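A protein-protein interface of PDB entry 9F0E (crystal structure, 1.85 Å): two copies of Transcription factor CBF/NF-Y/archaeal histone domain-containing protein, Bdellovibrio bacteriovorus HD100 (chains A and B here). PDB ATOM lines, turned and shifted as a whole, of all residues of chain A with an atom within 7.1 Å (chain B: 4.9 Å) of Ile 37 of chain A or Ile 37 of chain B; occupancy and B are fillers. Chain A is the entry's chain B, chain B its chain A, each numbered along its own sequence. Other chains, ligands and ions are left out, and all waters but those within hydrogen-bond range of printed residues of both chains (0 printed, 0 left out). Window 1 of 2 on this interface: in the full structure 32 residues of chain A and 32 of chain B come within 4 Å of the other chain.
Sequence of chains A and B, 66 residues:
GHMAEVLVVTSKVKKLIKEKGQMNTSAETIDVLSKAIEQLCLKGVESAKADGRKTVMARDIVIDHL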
ATOM      1  N   LEU A   7     -20.407  13.743   4.220  1.00  0.00           N
ATOM      2  CA  LEU A   7     -21.732  13.059   4.174  1.00  0.00           C
ATOM      3  C   LEU A   7     -21.833  12.131   2.955  1.00  0.00           C
ATOM      4  O   LEU A   7     -22.878  11.492   2.832  1.00  0.00           O
ATOM      5  CB  LEU A   7     -22.847  14.109   4.129  1.00  0.00           C
ATOM      6  CG  LEU A   7     -22.858  15.089   5.301  1.00  0.00           C
ATOM      7  CD1 LEU A   7     -23.858  16.219   5.056  1.00  0.00           C
ATOM      8  CD2 LEU A   7     -23.157  14.356   6.594  1.00  0.00           C
ATOM      9  N   VAL A   8     -20.823  12.077   2.073  1.00  0.00           N
ATOM     10  CA  VAL A   8     -20.793  11.112   0.927  1.00  0.00           C
ATOM     11  C   VAL A   8     -19.792   9.995   1.233  1.00  0.00           C
ATOM     12  O   VAL A   8     -18.833  10.245   2.015  1.00  0.00           O
ATOM     13  CB  VAL A   8     -20.458  11.765  -0.419  1.00  0.00           C
ATOM     14  CG1 VAL A   8     -21.568  12.694  -0.883  1.00  0.00           C
ATOM     15  CG2 VAL A   8     -19.095  12.453  -0.406  1.00  0.00           C
ATOM     16  N   VAL A   9     -20.007   8.814   0.636  1.00  0.00           N
ATOM     17  CA  VAL A   9     -19.076   7.655   0.746  1.00  0.00           C
ATOM     18  C   VAL A   9     -18.011   7.860  -0.341  1.00  0.00           C
ATOM     19  O   VAL A   9     -18.267   7.505  -1.519  1.00  0.00           O
ATOM     20  CB  VAL A   9     -19.791   6.291   0.639  1.00  0.00           C
ATOM     21  CG1 VAL A   9     -18.828   5.138   0.897  1.00  0.00           C
ATOM     22  CG2 VAL A   9     -20.979   6.188   1.595  1.00  0.00           C
ATOM     23  N   VAL A  13     -18.027   7.008  -4.463  1.00  0.00           N
ATOM     24  CA  VAL A  13     -18.164   8.114  -5.459  1.00  0.00           C
ATOM     25  C   VAL A  13     -16.978   8.023  -6.442  1.00  0.00           C
ATOM     26  O   VAL A  13     -17.204   8.150  -7.662  1.00  0.00           O
ATOM     27  CB  VAL A  13     -18.244   9.502  -4.792  1.00  0.00           C
ATOM     28  CG1 VAL A  13     -17.888  10.620  -5.752  1.00  0.00           C
ATOM     29  CG2 VAL A  13     -19.601   9.748  -4.155  1.00  0.00           C
ATOM     30  N   LEU A  16     -17.385   4.992  -8.784  1.00  0.00           N
ATOM     31  CA  LEU A  16     -18.431   5.320  -9.791  1.00  0.00           C
ATOM     32  C   LEU A  16     -17.844   6.192 -10.908  1.00  0.00           C
ATOM     33  O   LEU A  16     -18.079   5.899 -12.107  1.00  0.00           O
ATOM     34  CB  LEU A  16     -19.594   6.049  -9.117  1.00  0.00           C
ATOM     35  CG  LEU A  16     -20.613   6.632 -10.090  1.00  0.00           C
ATOM     36  CD1 LEU A  16     -21.297   5.512 -10.871  1.00  0.00           C
ATOM     37  CD2 LEU A  16     -21.631   7.475  -9.344  1.00  0.00           C
ATOM     38  N   ASP A  31     -15.980  17.536  -1.486  1.00  0.00           N
ATOM     39  CA  ASP A  31     -16.459  18.626  -0.597  1.00  0.00           C
ATOM     40  C   ASP A  31     -17.766  19.205  -1.146  1.00  0.00           C
ATOM     41  O   ASP A  31     -18.652  19.446  -0.346  1.00  0.00           O
ATOM     42  CB  ASP A  31     -15.429  19.742  -0.443  1.00  0.00           C
ATOM     43  CG  ASP A  31     -14.178  19.332   0.316  1.00  0.00           C
ATOM     44  OD1 ASP A  31     -14.166  18.234   0.894  1.00  0.00           O
ATOM     45  OD2 ASP A  31     -13.223  20.107   0.304  1.00  0.00           O
ATOM     46  N   VAL A  32     -17.884  19.430  -2.458  1.00  0.00           N
ATOM     47  CA  VAL A  32     -19.117  20.031  -3.057  1.00  0.00           C
ATOM     48  C   VAL A  32     -20.267  19.024  -2.879  1.00  0.00           C
ATOM     49  O   VAL A  32     -21.383  19.466  -2.555  1.00  0.00           O
ATOM     50  CB  VAL A  32     -18.951  20.438  -4.538  1.00  0.00           C
ATOM     51  CG1 VAL A  32     -20.246  21.031  -5.090  1.00  0.00           C
ATOM     52  CG2 VAL A  32     -17.801  21.408  -4.765  1.00  0.00           C
ATOM     53  N   LEU A  33     -19.999  17.721  -3.044  1.00  0.00           N
ATOM     54  CA  LEU A  33     -21.031  16.655  -2.938  1.00  0.00           C
ATOM     55  C   LEU A  33     -21.535  16.586  -1.486  1.00  0.00           C
ATOM     56  O   LEU A  33     -22.749  16.493  -1.332  1.00  0.00           O
ATOM     57  CB  LEU A  33     -20.465  15.318  -3.408  1.00  0.00           C
ATOM     58  CG  LEU A  33     -20.145  15.245  -4.899  1.00  0.00           C
ATOM     59  CD1 LEU A  33     -19.430  13.947  -5.201  1.00  0.00           C
ATOM     60  CD2 LEU A  33     -21.417  15.372  -5.729  1.00  0.00           C
ATOM     61  N   SER A  34     -20.639  16.678  -0.495  1.00  0.00           N
ATOM     62  CA  SER A  34     -20.989  16.727   0.945  1.00  0.00           C
ATOM     63  C   SER A  34     -21.836  17.975   1.246  1.00  0.00           C
ATOM     64  O   SER A  34     -22.897  17.824   1.906  1.00  0.00           O
ATOM     65  CB  SER A  34     -19.759  16.666   1.787  1.00  0.00           C
ATOM     66  OG  SER A  34     -20.094  16.322   3.111  1.00  0.00           O
ATOM     67  N   LYS A  35     -21.398  19.151   0.789  1.00  0.00           N
ATOM     68  CA  LYS A  35     -22.154  20.424   0.962  1.00  0.00           C
ATOM     69  C   LYS A  35     -23.525  20.309   0.289  1.00  0.00           C
ATOM     70  O   LYS A  35     -24.516  20.794   0.878  1.00  0.00           O
ATOM     71  CB  LYS A  35     -21.417  21.623   0.366  1.00  0.00           C
ATOM     72  CG  LYS A  35     -22.141  22.956   0.528  1.00  0.00           C
ATOM     73  CD  LYS A  35     -21.815  23.702   1.813  1.00  0.00           C
ATOM     74  CE  LYS A  35     -22.787  24.821   2.161  1.00  0.00           C
ATOM     75  NZ  LYS A  35     -23.721  25.140   1.049  1.00  0.00           N
ATOM     76  N   ALA A  36     -23.607  19.652  -0.877  1.00  0.00           N
ATOM     77  CA  ALA A  36     -24.888  19.476  -1.592  1.00  0.00           C
ATOM     78  C   ALA A  36     -25.840  18.617  -0.739  1.00  0.00           C
ATOM     79  O   ALA A  36     -27.015  18.996  -0.626  1.00  0.00           O
ATOM     80  CB  ALA A  36     -24.654  18.896  -2.969  1.00  0.00           C
ATOM     81  N   ILE A  37     -25.362  17.521  -0.134  1.00  0.00           N
ATOM     82  CA  ILE A  37     -26.182  16.638   0.751  1.00  0.00           C
ATOM     83  C   ILE A  37     -26.664  17.479   1.941  1.00  0.00           C
ATOM     84  O   ILE A  37     -27.858  17.398   2.297  1.00  0.00           O
ATOM     85  CB  ILE A  37     -25.403  15.382   1.213  1.00  0.00           C
ATOM     86  CG1 ILE A  37     -25.055  14.452   0.051  1.00  0.00           C
ATOM     87  CG2 ILE A  37     -26.173  14.611   2.277  1.00  0.00           C
ATOM     88  CD1 ILE A  37     -26.230  14.110  -0.826  1.00  0.00           C
ATOM     89  N   GLU A  38     -25.764  18.233   2.565  1.00  0.00           N
ATOM     90  CA  GLU A  38     -26.093  19.089   3.739  1.00  0.00           C
ATOM     91  C   GLU A  38     -27.264  20.014   3.390  1.00  0.00           C
ATOM     92  O   GLU A  38     -28.247  20.059   4.192  1.00  0.00           O
ATOM     93  CB  GLU A  38     -24.889  19.921   4.182  1.00  0.00           C
ATOM     94  CG  GLU A  38     -25.163  20.770   5.411  1.00  0.00           C
ATOM     95  CD  GLU A  38     -24.029  21.679   5.831  1.00  0.00           C
ATOM     96  OE1 GLU A  38     -23.499  22.407   4.978  1.00  0.00           O
ATOM     97  OE2 GLU A  38     -23.662  21.633   7.013  1.00  0.00           O
ATOM     98  N   GLN A  39     -27.170  20.743   2.272  1.00  0.00           N
ATOM     99  CA  GLN A  39     -28.202  21.729   1.865  1.00  0.00           C
ATOM    100  C   GLN A  39     -29.514  20.995   1.540  1.00  0.00           C
ATOM    101  O   GLN A  39     -30.585  21.477   1.986  1.00  0.00           O
ATOM    102  CB  GLN A  39     -27.710  22.619   0.731  1.00  0.00           C
ATOM    103  CG  GLN A  39     -26.648  23.617   1.179  1.00  0.00           C
ATOM    104  CD  GLN A  39     -27.116  24.507   2.313  1.00  0.00           C
ATOM    105  OE1 GLN A  39     -28.109  25.207   2.199  1.00  0.00           O
ATOM    106  NE2 GLN A  39     -26.380  24.530   3.412  1.00  0.00           N
ATOM    107  N   LEU A  40     -29.460  19.838   0.890  1.00  0.00           N
ATOM    108  CA  LEU A  40     -30.713  19.058   0.639  1.00  0.00           C
ATOM    109  C   LEU A  40     -31.385  18.651   1.954  1.00  0.00           C
ATOM    110  O   LEU A  40     -32.638  18.748   2.028  1.00  0.00           O
ATOM    111  CB  LEU A  40     -30.392  17.829  -0.204  1.00  0.00           C
ATOM    112  CG  LEU A  40     -30.102  18.135  -1.667  1.00  0.00           C
ATOM    113  CD1 LEU A  40     -29.643  16.893  -2.399  1.00  0.00           C
ATOM    114  CD2 LEU A  40     -31.312  18.745  -2.367  1.00  0.00           C
ATOM    115  N   CYS A  41     -30.617  18.167   2.939  1.00  0.00           N
ATOM    116  CA  CYS A  41     -31.147  17.739   4.259  1.00  0.00           C
ATOM    117  C   CYS A  41     -31.763  18.930   5.007  1.00  0.00           C
ATOM    118  O   CYS A  41     -32.866  18.750   5.610  1.00  0.00           O
ATOM    119  CB  CYS A  41     -30.092  17.100   5.152  1.00  0.00           C
ATOM    120  SG  CYS A  41     -29.452  15.517   4.564  1.00  0.00           S
ATOM    121  N   LEU A  42     -31.080  20.081   5.053  1.00  0.00           N
ATOM    122  CA  LEU A  42     -31.595  21.289   5.742  1.00  0.00           C
ATOM    123  C   LEU A  42     -32.879  21.792   5.059  1.00  0.00           C
ATOM    124  O   LEU A  42     -33.814  22.167   5.789  1.00  0.00           O
ATOM    125  CB  LEU A  42     -30.500  22.361   5.817  1.00  0.00           C
ATOM    126  CG  LEU A  42     -29.312  21.984   6.696  1.00  0.00           C
ATOM    127  CD1 LEU A  42     -28.224  23.042   6.624  1.00  0.00           C
ATOM    128  CD2 LEU A  42     -29.782  21.762   8.132  1.00  0.00           C
ATOM    129  N   LYS A  43     -32.951  21.790   3.730  1.00  0.00           N
ATOM    130  CA  LYS A  43     -34.187  22.190   2.992  1.00  0.00           C
ATOM    131  C   LYS A  43     -35.294  21.154   3.232  1.00  0.00           C
ATOM    132  O   LYS A  43     -36.501  21.561   3.259  1.00  0.00           O
ATOM    133  CB  LYS A  43     -33.885  22.395   1.503  1.00  0.00           C
ATOM    134  CG  LYS A  43     -33.215  23.737   1.203  1.00  0.00           C
ATOM    135  N   ILE A  61     -37.203  16.221  -0.268  1.00  0.00           N
ATOM    136  CA  ILE A  61     -35.903  16.450  -0.969  1.00  0.00           C
ATOM    137  C   ILE A  61     -36.220  16.862  -2.408  1.00  0.00           C
ATOM    138  O   ILE A  61     -36.463  15.954  -3.269  1.00  0.00           O
ATOM    139  CB  ILE A  61     -35.012  15.197  -0.924  1.00  0.00           C
ATOM    140  CG1 ILE A  61     -34.914  14.613   0.481  1.00  0.00           C
ATOM    141  CG2 ILE A  61     -33.640  15.488  -1.525  1.00  0.00           C
ATOM    142  CD1 ILE A  61     -34.426  15.593   1.540  1.00  0.00           C
ATOM    143  N   LEU B   7     -24.604   5.933  -1.712  1.00  0.00           N
ATOM    144  CA  LEU B   7     -23.478   6.896  -1.869  1.00  0.00           C
ATOM    145  C   LEU B   7     -23.437   7.916  -0.730  1.00  0.00           C
ATOM    146  O   LEU B   7     -22.511   8.717  -0.743  1.00  0.00           O
ATOM    147  CB  LEU B   7     -23.597   7.588  -3.228  1.00  0.00           C
ATOM    148  CG  LEU B   7     -23.559   6.633  -4.421  1.00  0.00           C
ATOM    149  CD1 LEU B   7     -23.883   7.353  -5.713  1.00  0.00           C
ATOM    150  CD2 LEU B   7     -22.213   5.943  -4.519  1.00  0.00           C
ATOM    151  N   VAL B   8     -24.388   7.899   0.207  1.00  0.00           N
ATOM    152  CA  VAL B   8     -24.406   8.836   1.382  1.00  0.00           C
ATOM    153  C   VAL B   8     -24.096   8.036   2.645  1.00  0.00           C
ATOM    154  O   VAL B   8     -24.408   6.819   2.669  1.00  0.00           O
ATOM    155  CB  VAL B   8     -25.719   9.618   1.550  1.00  0.00           C
ATOM    156  CG1 VAL B   8     -25.972  10.580   0.396  1.00  0.00           C
ATOM    157  CG2 VAL B   8     -26.916   8.697   1.758  1.00  0.00           C
ATOM    158  N   VAL B  13     -26.142  11.486   7.983  1.00  0.00           N
ATOM    159  CA  VAL B  13     -27.314  12.242   7.442  1.00  0.00           C
ATOM    160  C   VAL B  13     -28.408  12.251   8.525  1.00  0.00           C
ATOM    161  O   VAL B  13     -29.017  13.324   8.766  1.00  0.00           O
ATOM    162  CB  VAL B  13     -27.835  11.655   6.112  1.00  0.00           C
ATOM    163  CG1 VAL B  13     -29.252  12.118   5.809  1.00  0.00           C
ATOM    164  CG2 VAL B  13     -26.912  11.968   4.937  1.00  0.00           C
ATOM    165  N   LEU B  33     -31.277  10.873  -1.696  1.00  0.00           N
ATOM    166  CA  LEU B  33     -29.961  11.545  -1.499  1.00  0.00           C
ATOM    167  C   LEU B  33     -28.883  10.779  -2.279  1.00  0.00           C
ATOM    168  O   LEU B  33     -28.067  11.452  -2.931  1.00  0.00           O
ATOM    169  CB  LEU B  33     -29.637  11.653  -0.009  1.00  0.00           C
ATOM    170  CG  LEU B  33     -30.544  12.615   0.762  1.00  0.00           C
ATOM    171  CD1 LEU B  33     -30.284  12.541   2.251  1.00  0.00           C
ATOM    172  CD2 LEU B  33     -30.364  14.047   0.263  1.00  0.00           C
ATOM    173  N   SER B  34     -28.900   9.444  -2.243  1.00  0.00           N
ATOM    174  CA  SER B  34     -27.959   8.572  -3.000  1.00  0.00           C
ATOM    175  C   SER B  34     -28.138   8.792  -4.510  1.00  0.00           C
ATOM    176  O   SER B  34     -27.115   8.988  -5.204  1.00  0.00           O
ATOM    177  CB  SER B  34     -28.141   7.120  -2.635  1.00  0.00           C
ATOM    178  OG  SER B  34     -27.334   6.758  -1.529  1.00  0.00           O
ATOM    179  N   LYS B  35     -29.384   8.765  -5.001  1.00  0.00           N
ATOM    180  CA  LYS B  35     -29.699   8.994  -6.438  1.00  0.00           C
ATOM    181  C   LYS B  35     -29.258  10.405  -6.819  1.00  0.00           C
ATOM    182  O   LYS B  35     -28.733  10.576  -7.946  1.00  0.00           O
ATOM    183  CB  LYS B  35     -31.190   8.818  -6.750  1.00  0.00           C
ATOM    184  N   ALA B  36     -29.418  11.390  -5.927  1.00  0.00           N
ATOM    185  CA  ALA B  36     -28.990  12.777  -6.221  1.00  0.00           C
ATOM    186  C   ALA B  36     -27.460  12.825  -6.405  1.00  0.00           C
ATOM    187  O   ALA B  36     -27.011  13.472  -7.371  1.00  0.00           O
ATOM    188  CB  ALA B  36     -29.506  13.711  -5.153  1.00  0.00           C
ATOM    189  N   ILE B  37     -26.678  12.165  -5.540  1.00  0.00           N
ATOM    190  CA  ILE B  37     -25.190  12.084  -5.656  1.00  0.00           C
ATOM    191  C   ILE B  37     -24.840  11.408  -6.992  1.00  0.00           C
ATOM    192  O   ILE B  37     -23.946  11.906  -7.709  1.00  0.00           O
ATOM    193  CB  ILE B  37     -24.555  11.338  -4.456  1.00  0.00           C
ATOM    194  CG1 ILE B  37     -24.749  12.102  -3.145  1.00  0.00           C
ATOM    195  CG2 ILE B  37     -23.073  11.068  -4.683  1.00  0.00           C
ATOM    196  CD1 ILE B  37     -24.251  13.518  -3.223  1.00  0.00           C
ATOM    197  N   GLU B  38     -25.470  10.282  -7.300  1.00  0.00           N
ATOM    198  CA  GLU B  38     -25.236   9.540  -8.569  1.00  0.00           C
ATOM    199  C   GLU B  38     -25.386  10.480  -9.770  1.00  0.00           C
ATOM    200  O   GLU B  38     -24.448  10.507 -10.624  1.00  0.00           O
ATOM    201  CB  GLU B  38     -26.198   8.354  -8.708  1.00  0.00           C
ATOM    202  CG  GLU B  38     -25.933   7.517  -9.941  1.00  0.00           C
ATOM    203  CD  GLU B  38     -26.904   6.381 -10.168  1.00  0.00           C
ATOM    204  OE1 GLU B  38     -28.112   6.641 -10.194  1.00  0.00           O
ATOM    205  OE2 GLU B  38     -26.435   5.239 -10.347  1.00  0.00           O
ATOM    206  N   GLN B  39     -26.505  11.207  -9.855  1.00  0.00           N
ATOM    207  CA  GLN B  39     -26.786  12.104 -11.009  1.00  0.00           C
ATOM    208  C   GLN B  39     -25.778  13.265 -11.029  1.00  0.00           C
ATOM    209  O   GLN B  39     -25.281  13.595 -12.138  1.00  0.00           O
ATOM    210  CB  GLN B  39     -28.239  12.567 -11.000  1.00  0.00           C
ATOM    211  CG  GLN B  39     -29.227  11.444 -11.350  1.00  0.00           C
ATOM    212  CD  GLN B  39     -28.927  10.843 -12.712  1.00  0.00           C
ATOM    213  OE1 GLN B  39     -28.841  11.544 -13.712  1.00  0.00           O
ATOM    214  NE2 GLN B  39     -28.779   9.530 -12.766  1.00  0.00           N
ATOM    215  N   LEU B  40     -25.405  13.820  -9.879  1.00  0.00           N
ATOM    216  CA  LEU B  40     -24.358  14.888  -9.860  1.00  0.00           C
ATOM    217  C   LEU B  40     -23.024  14.369 -10.401  1.00  0.00           C
ATOM    218  O   LEU B  40     -22.380  15.108 -11.194  1.00  0.00           O
ATOM    219  CB  LEU B  40     -24.182  15.406  -8.434  1.00  0.00           C
ATOM    220  CG  LEU B  40     -25.308  16.299  -7.938  1.00  0.00           C
ATOM    221  CD1 LEU B  40     -25.099  16.669  -6.487  1.00  0.00           C
ATOM    222  CD2 LEU B  40     -25.474  17.546  -8.785  1.00  0.00           C
ATOM    223  N   CYS B  41     -22.600  13.164  -9.992  1.00  0.00           N
ATOM    224  CA  CYS B  41     -21.331  12.528 -10.451  1.00  0.00           C
ATOM    225  C   CYS B  41     -21.373  12.273 -11.961  1.00  0.00           C
ATOM    226  O   CYS B  41     -20.340  12.559 -12.644  1.00  0.00           O
ATOM    227  CB  CYS B  41     -21.024  11.227  -9.719  1.00  0.00           C
ATOM    228  SG  CYS B  41     -20.661  11.429  -7.950  1.00  0.00           S
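Of chain B, only Val 8 (3.7 Å), Val 13 (3.8 Å), Leu 33 (3.9 Å) and Ile 37 (3.2 Å) come within 4 Å of Ile 37 of chain A. Ile 37 of chain B touches just these residues of chain A: Val 8, Val 13, Leu 33 and Ile 37. Of the printed residues of chain A, Val 13 of chain B touches Ile 37 and Cys 41. Of the printed residues of chain B, Cys 41 of chain A touches Val 13 and Leu 33. Printed residues of chain A within 4 Å of Leu 40 of chain B: Leu 33. Of the printed residues of chain B, Val 9 of chain A touches Leu 7 (2.9 Å) and Val 8 (3.6 Å). The nearest printed residue of chain B that does not touch Ile 37 of chain A is Ala 36 of chain B (5.4 Å). The nearest residue of chain A that does not touch Ile 37 of chain B is Leu 16 of chain A (5.3 Å).
N of Val 9 of chain A is in hydrogen-bond range of O of Leu 7 of chain B, 2.9 Å away.
Of the 19 printed residues of chain A, 9 touch a printed residue of chain B. Hydrophobic or aromatic side chains of chain A that line the printed part of chain B: Val 8, Val 9, Val 13, Leu 16, Leu 33, Ile 37 and Leu 40. Hydrophobic or aromatic side chains of chain B within 4 Å of the printed part of chain A: Val 8, Val 13, Leu 33, Ile 37 and Leu 40. Among the printed residues, 18 pairs touch across the chains.
Among the printed residues, merely in contact across the chains: Leu 7 of chain A with Val 8 of chain B (3.4 Å), Val 8 of chain A with Leu 7 of chain B (3.4 Å), Val 8 of chain A with Ile 37 of chain B (3.7 Å), Val 9 of chain A with Val 8 of chain B (3.6 Å), Val 13 of chain A with Ile 37 of chain B (3.8 Å), Val 13 of chain A with Cys 41 of chain B (3.6 Å), Leu 16 of chain A with Cys 41 of chain B (3.8 Å), Leu 33 of chain A with Ile 37 of chain B (3.8 Å), Leu 33 of chain A with Leu 40 of chain B (3.9 Å), Leu 33 of chain A with Cys 41 of chain B (3.9 Å), Ile 37 of chain A with Val 8 of chain B (3.7 Å), Ile 37 of chain A with Val 13 of chain B (3.8 Å), Ile 37 of chain A with Leu 33 of chain B (3.9 Å), Ile 37 of chain A with Ile 37 of chain B (3.2 Å), Leu 40 of chain A with Leu 33 of chain B (3.8 Å), Cys 41 of chain A with Val 13 of chain B (3.6 Å) and Cys 41 of chain A with Leu 33 of chain B (3.9 Å).
Val 13 of chain A touches Cys 41 of chain B, and with the chains exchanged Cys 41 of chain A touches Val 13 of chain B. Leu 33 of chain A touches Ile 37 of chain B, and with the chains exchanged Ile 37 of chain A touches Leu 33 of chain B. Leu 33 of chain A touches Cys 41 of chain B, and with the chains exchanged Cys 41 of chain A touches Leu 33 of chain B. Ile 37 of chain B touches its own counterpart, Ile 37 of chain A.
SG of Cys 41 of chain B lies within hydrogen-bond range of O of Ile 37 of chain B (3.3 Å). N of Leu 7 of chain A sits at hydrogen-bond distance from OG of Ser 34 of chain A (2.8 Å). The side-chain hydroxyl (OG) of Ser 34 of chain B lies within hydrogen-bond range of the backbone NH (N) of Leu 7 of chain B (2.9 Å). The side-chain sulfur (SG) of Cys 41 of chain A lies within hydrogen-bond range of the backbone carbonyl oxygen (O) of Ile 37 of chain A (3.3 Å).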
